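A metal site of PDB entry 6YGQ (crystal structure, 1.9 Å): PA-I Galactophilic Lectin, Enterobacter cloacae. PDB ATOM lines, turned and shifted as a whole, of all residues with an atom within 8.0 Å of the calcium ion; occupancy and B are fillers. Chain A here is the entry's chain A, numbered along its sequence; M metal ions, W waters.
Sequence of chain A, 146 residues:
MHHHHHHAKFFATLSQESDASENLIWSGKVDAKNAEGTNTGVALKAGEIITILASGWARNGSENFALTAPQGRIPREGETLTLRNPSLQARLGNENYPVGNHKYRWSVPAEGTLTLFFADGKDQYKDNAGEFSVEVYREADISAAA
ND2 of Asn 128 sits at hydrogen-bond distance from O of Ala 32 (2.9 Å).
The backbone carbonyl oxygen (O) of Tyr 125 lies close to the side-chain amide nitrogen (ND2) of Asn 128 (3.3 Å).
OH of Tyr 125 is in hydrogen-bond range of N of Asp 120, at 3.0 Å.
O of Ala 66 sits at hydrogen-bond distance from N of Asn 60 (3.0 Å).
Of the 19 residues printed, 5 come within 4 Å of the calcium ion.
The calcium ion is bound by O of Gln 124 (2.3 Å), OD1 of Asn 128 (2.4 Å), O of Asn 60 (2.4 Å), OD1 of Asp 127 (2.4 Å), water W2 (2.5 Å), OD2 of Asp 120 (2.5 Å) and water W1 (2.5 Å).
The calcium ion has seven donor atoms within binding distance.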
ATOM      1  N   ALA A  32     -25.040  22.270 -30.679  1.00  0.00           N
ATOM      2  CA  ALA A  32     -25.926  22.549 -29.553  1.00  0.00           C
ATOM      3  C   ALA A  32     -25.396  23.660 -28.651  1.00  0.00           C
ATOM      4  O   ALA A  32     -26.179  24.242 -27.884  1.00  0.00           O
ATOM      5  CB  ALA A  32     -26.130  21.277 -28.723  1.00  0.00           C
ATOM      6  N   LYS A  33     -24.103  23.973 -28.725  1.00  0.00           N
ATOM      7  CA  LYS A  33     -23.493  24.978 -27.870  1.00  0.00           C
ATOM      8  C   LYS A  33     -23.473  26.375 -28.500  1.00  0.00           C
ATOM      9  O   LYS A  33     -23.024  27.317 -27.846  1.00  0.00           O
ATOM     10  CB  LYS A  33     -22.057  24.567 -27.524  1.00  0.00           C
ATOM     11  CG  LYS A  33     -21.930  23.789 -26.224  1.00  0.00           C
ATOM     12  CD  LYS A  33     -21.053  22.551 -26.359  1.00  0.00           C
ATOM     13  CE  LYS A  33     -19.696  22.858 -26.971  1.00  0.00           C
ATOM     14  NZ  LYS A  33     -18.672  21.860 -26.559  1.00  0.00           N
ATOM     15  N   ARG A  59     -27.220  17.211 -25.938  1.00  0.00           N
ATOM     16  CA  ARG A  59     -27.532  17.442 -24.531  1.00  0.00           C
ATOM     17  C   ARG A  59     -27.659  18.935 -24.284  1.00  0.00           C
ATOM     18  O   ARG A  59     -26.820  19.723 -24.746  1.00  0.00           O
ATOM     19  CB  ARG A  59     -26.460  16.844 -23.625  1.00  0.00           C
ATOM     20  CG  ARG A  59     -26.363  15.327 -23.693  1.00  0.00           C
ATOM     21  CD  ARG A  59     -24.951  14.856 -23.400  1.00  0.00           C
ATOM     22  NE  ARG A  59     -24.612  14.976 -21.986  1.00  0.00           N
ATOM     23  CZ  ARG A  59     -23.384  15.220 -21.520  1.00  0.00           C
ATOM     24  NH1 ARG A  59     -22.365  15.382 -22.352  1.00  0.00           N
ATOM     25  NH2 ARG A  59     -23.177  15.313 -20.208  1.00  0.00           N
ATOM     26  N   ASN A  60     -28.709  19.337 -23.553  1.00  0.00           N
ATOM     27  CA  ASN A  60     -28.864  20.719 -23.134  1.00  0.00           C
ATOM     28  C   ASN A  60     -28.359  20.943 -21.706  1.00  0.00           C
ATOM     29  O   ASN A  60     -28.606  22.004 -21.126  1.00  0.00           O
ATOM     30  CB  ASN A  60     -30.329  21.169 -23.255  1.00  0.00           C
ATOM     31  CG  ASN A  60     -31.286  20.288 -22.459  1.00  0.00           C
ATOM     32  OD1 ASN A  60     -30.869  19.464 -21.643  1.00  0.00           O
ATOM     33  ND2 ASN A  60     -32.575  20.480 -22.684  1.00  0.00           N
ATOM     34  N   GLY A  61     -27.637  19.975 -21.150  1.00  0.00           N
ATOM     35  CA  GLY A  61     -27.083  20.099 -19.818  1.00  0.00           C
ATOM     36  C   GLY A  61     -26.175  18.922 -19.542  1.00  0.00           C
ATOM     37  O   GLY A  61     -26.018  18.020 -20.380  1.00  0.00           O
ATOM     38  N   SER A  62     -25.580  18.923 -18.351  1.00  0.00           N
ATOM     39  CA  SER A  62     -24.655  17.873 -17.966  1.00  0.00           C
ATOM     40  C   SER A  62     -25.339  16.650 -17.369  1.00  0.00           C
ATOM     41  O   SER A  62     -24.720  15.577 -17.324  1.00  0.00           O
ATOM     42  CB  SER A  62     -23.630  18.410 -16.955  1.00  0.00           C
ATOM     43  OG  SER A  62     -22.834  19.443 -17.526  1.00  0.00           O
ATOM     44  N   GLU A  63     -26.578  16.779 -16.915  1.00  0.00           N
ATOM     45  CA  GLU A  63     -27.265  15.671 -16.273  1.00  0.00           C
ATOM     46  C   GLU A  63     -27.646  14.604 -17.295  1.00  0.00           C
ATOM     47  O   GLU A  63     -27.821  14.882 -18.487  1.00  0.00           O
ATOM     48  CB  GLU A  63     -28.513  16.159 -15.545  1.00  0.00           C
ATOM     49  CG  GLU A  63     -28.267  17.287 -14.554  1.00  0.00           C
ATOM     50  CD  GLU A  63     -28.493  18.651 -15.170  1.00  0.00           C
ATOM     51  OE1 GLU A  63     -29.016  19.544 -14.460  1.00  0.00           O
ATOM     52  OE2 GLU A  63     -28.159  18.843 -16.363  1.00  0.00           O
ATOM     53  N   ALA A  66     -30.596  15.235 -19.438  1.00  0.00           N
ATOM     54  CA  ALA A  66     -30.564  16.470 -20.227  1.00  0.00           C
ATOM     55  C   ALA A  66     -30.237  16.167 -21.691  1.00  0.00           C
ATOM     56  O   ALA A  66     -29.283  16.680 -22.269  1.00  0.00           O
ATOM     57  CB  ALA A  66     -29.552  17.447 -19.632  1.00  0.00           C
ATOM     58  N   PHE A 118     -29.988  25.408 -32.359  1.00  0.00           N
ATOM     59  CA  PHE A 118     -30.449  24.607 -31.231  1.00  0.00           C
ATOM     60  C   PHE A 118     -31.074  25.546 -30.199  1.00  0.00           C
ATOM     61  O   PHE A 118     -30.475  26.562 -29.832  1.00  0.00           O
ATOM     62  CB  PHE A 118     -29.278  23.838 -30.623  1.00  0.00           C
ATOM     63  CG  PHE A 118     -29.646  22.976 -29.440  1.00  0.00           C
ATOM     64  CD1 PHE A 118     -29.505  23.459 -28.144  1.00  0.00           C
ATOM     65  CD2 PHE A 118     -30.118  21.693 -29.624  1.00  0.00           C
ATOM     66  CE1 PHE A 118     -29.831  22.673 -27.059  1.00  0.00           C
ATOM     67  CE2 PHE A 118     -30.458  20.904 -28.540  1.00  0.00           C
ATOM     68  CZ  PHE A 118     -30.312  21.397 -27.252  1.00  0.00           C
ATOM     69  N   ALA A 119     -32.283  25.217 -29.753  1.00  0.00           N
ATOM     70  CA  ALA A 119     -33.036  26.070 -28.846  1.00  0.00           C
ATOM     71  C   ALA A 119     -32.625  25.806 -27.407  1.00  0.00           C
ATOM     72  O   ALA A 119     -32.743  24.673 -26.920  1.00  0.00           O
ATOM     73  CB  ALA A 119     -34.535  25.846 -29.030  1.00  0.00           C
ATOM     74  N   ASP A 120     -32.167  26.847 -26.721  1.00  0.00           N
ATOM     75  CA  ASP A 120     -31.848  26.747 -25.303  1.00  0.00           C
ATOM     76  C   ASP A 120     -31.983  28.143 -24.697  1.00  0.00           C
ATOM     77  O   ASP A 120     -32.098  29.145 -25.407  1.00  0.00           O
ATOM     78  CB  ASP A 120     -30.438  26.182 -25.082  1.00  0.00           C
ATOM     79  CG  ASP A 120     -30.258  25.606 -23.679  1.00  0.00           C
ATOM     80  OD1 ASP A 120     -31.234  25.583 -22.901  1.00  0.00           O
ATOM     81  OD2 ASP A 120     -29.131  25.154 -23.369  1.00  0.00           O
ATOM     82  N   GLY A 121     -31.975  28.183 -23.367  1.00  0.00           N
ATOM     83  CA  GLY A 121     -32.120  29.449 -22.687  1.00  0.00           C
ATOM     84  C   GLY A 121     -30.939  30.371 -22.942  1.00  0.00           C
ATOM     85  O   GLY A 121     -29.801  29.932 -23.131  1.00  0.00           O
ATOM     86  N   ASP A 123     -27.855  32.400 -22.461  1.00  0.00           N
ATOM     87  CA  ASP A 123     -26.701  32.239 -21.577  1.00  0.00           C
ATOM     88  C   ASP A 123     -26.675  30.895 -20.876  1.00  0.00           C
ATOM     89  O   ASP A 123     -26.068  30.763 -19.807  1.00  0.00           O
ATOM     90  CB  ASP A 123     -26.629  33.366 -20.548  1.00  0.00           C
ATOM     91  CG  ASP A 123     -26.392  34.726 -21.176  1.00  0.00           C
ATOM     92  OD1 ASP A 123     -25.547  34.825 -22.085  1.00  0.00           O
ATOM     93  OD2 ASP A 123     -27.062  35.701 -20.769  1.00  0.00           O
ATOM     94  N   GLN A 124     -27.333  29.882 -21.444  1.00  0.00           N
ATOM     95  CA  GLN A 124     -27.305  28.529 -20.899  1.00  0.00           C
ATOM     96  C   GLN A 124     -26.809  27.519 -21.930  1.00  0.00           C
ATOM     97  O   GLN A 124     -27.036  26.312 -21.771  1.00  0.00           O
ATOM     98  CB  GLN A 124     -28.696  28.140 -20.386  1.00  0.00           C
ATOM     99  CG  GLN A 124     -29.190  29.005 -19.233  1.00  0.00           C
ATOM    100  CD  GLN A 124     -30.575  28.617 -18.750  1.00  0.00           C
ATOM    101  OE1 GLN A 124     -31.447  28.253 -19.536  1.00  0.00           O
ATOM    102  NE2 GLN A 124     -30.787  28.713 -17.439  1.00  0.00           N
ATOM    103  N   TYR A 125     -26.127  27.983 -22.967  1.00  0.00           N
ATOM    104  CA  TYR A 125     -25.738  27.105 -24.057  1.00  0.00           C
ATOM    105  C   TYR A 125     -24.446  26.342 -23.791  1.00  0.00           C
ATOM    106  O   TYR A 125     -24.241  25.275 -24.380  1.00  0.00           O
ATOM    107  CB  TYR A 125     -25.560  27.909 -25.356  1.00  0.00           C
ATOM    108  CG  TYR A 125     -26.822  28.101 -26.146  1.00  0.00           C
ATOM    109  CD1 TYR A 125     -27.706  29.131 -25.851  1.00  0.00           C
ATOM    110  CD2 TYR A 125     -27.140  27.255 -27.206  1.00  0.00           C
ATOM    111  CE1 TYR A 125     -28.864  29.313 -26.566  1.00  0.00           C
ATOM    112  CE2 TYR A 125     -28.305  27.433 -27.942  1.00  0.00           C
ATOM    113  CZ  TYR A 125     -29.160  28.462 -27.618  1.00  0.00           C
ATOM    114  OH  TYR A 125     -30.312  28.652 -28.332  1.00  0.00           O
ATOM    115  N   LYS A 126     -23.580  26.842 -22.924  1.00  0.00           N
ATOM    116  CA  LYS A 126     -22.202  26.359 -22.899  1.00  0.00           C
ATOM    117  C   LYS A 126     -22.005  25.135 -22.016  1.00  0.00           C
ATOM    118  O   LYS A 126     -20.868  24.664 -21.905  1.00  0.00           O
ATOM    119  CB  LYS A 126     -21.268  27.502 -22.459  1.00  0.00           C
ATOM    120  CG  LYS A 126     -21.212  28.653 -23.472  1.00  0.00           C
ATOM    121  CD  LYS A 126     -21.014  28.136 -24.894  1.00  0.00           C
ATOM    122  CE  LYS A 126     -20.765  29.263 -25.891  1.00  0.00           C
ATOM    123  NZ  LYS A 126     -20.411  28.724 -27.233  1.00  0.00           N
ATOM    124  N   ASP A 127     -23.061  24.590 -21.419  1.00  0.00           N
ATOM    125  CA  ASP A 127     -23.007  23.252 -20.851  1.00  0.00           C
ATOM    126  C   ASP A 127     -23.683  22.214 -21.751  1.00  0.00           C
ATOM    127  O   ASP A 127     -23.925  21.088 -21.308  1.00  0.00           O
ATOM    128  CB  ASP A 127     -23.642  23.226 -19.454  1.00  0.00           C
ATOM    129  CG  ASP A 127     -25.104  23.594 -19.470  1.00  0.00           C
ATOM    130  OD1 ASP A 127     -25.663  23.843 -20.558  1.00  0.00           O
ATOM    131  OD2 ASP A 127     -25.703  23.635 -18.368  1.00  0.00           O
ATOM    132  N   ASN A 128     -23.978  22.582 -22.989  1.00  0.00           N
ATOM    133  CA  ASN A 128     -24.603  21.650 -23.920  1.00  0.00           C
ATOM    134  C   ASN A 128     -23.542  20.776 -24.579  1.00  0.00           C
ATOM    135  O   ASN A 128     -22.341  20.906 -24.320  1.00  0.00           O
ATOM    136  CB  ASN A 128     -25.413  22.415 -24.966  1.00  0.00           C
ATOM    137  CG  ASN A 128     -26.554  23.193 -24.345  1.00  0.00           C
ATOM    138  OD1 ASN A 128     -26.831  23.074 -23.159  1.00  0.00           O
ATOM    139  ND2 ASN A 128     -27.224  24.015 -25.159  1.00  0.00           N
ATOM    140  N   ALA A 129     -23.998  19.862 -25.432  1.00  0.00           N
ATOM    141  CA  ALA A 129     -23.088  18.949 -26.123  1.00  0.00           C
ATOM    142  C   ALA A 129     -23.812  18.352 -27.315  1.00  0.00           C
ATOM    143  O   ALA A 129     -25.044  18.271 -27.326  1.00  0.00           O
ATOM    144  CB  ALA A 129     -22.590  17.842 -25.188  1.00  0.00           C
HETATM  145 CA    CA M   1     -27.896  24.262 -21.407  1.00  0.00          CA
HETATM  146  O   HOH W   1     -28.016  24.410 -18.870  1.00  0.00           O
HETATM  147  O   HOH W   2     -30.211  24.710 -20.659  1.00  0.00           O
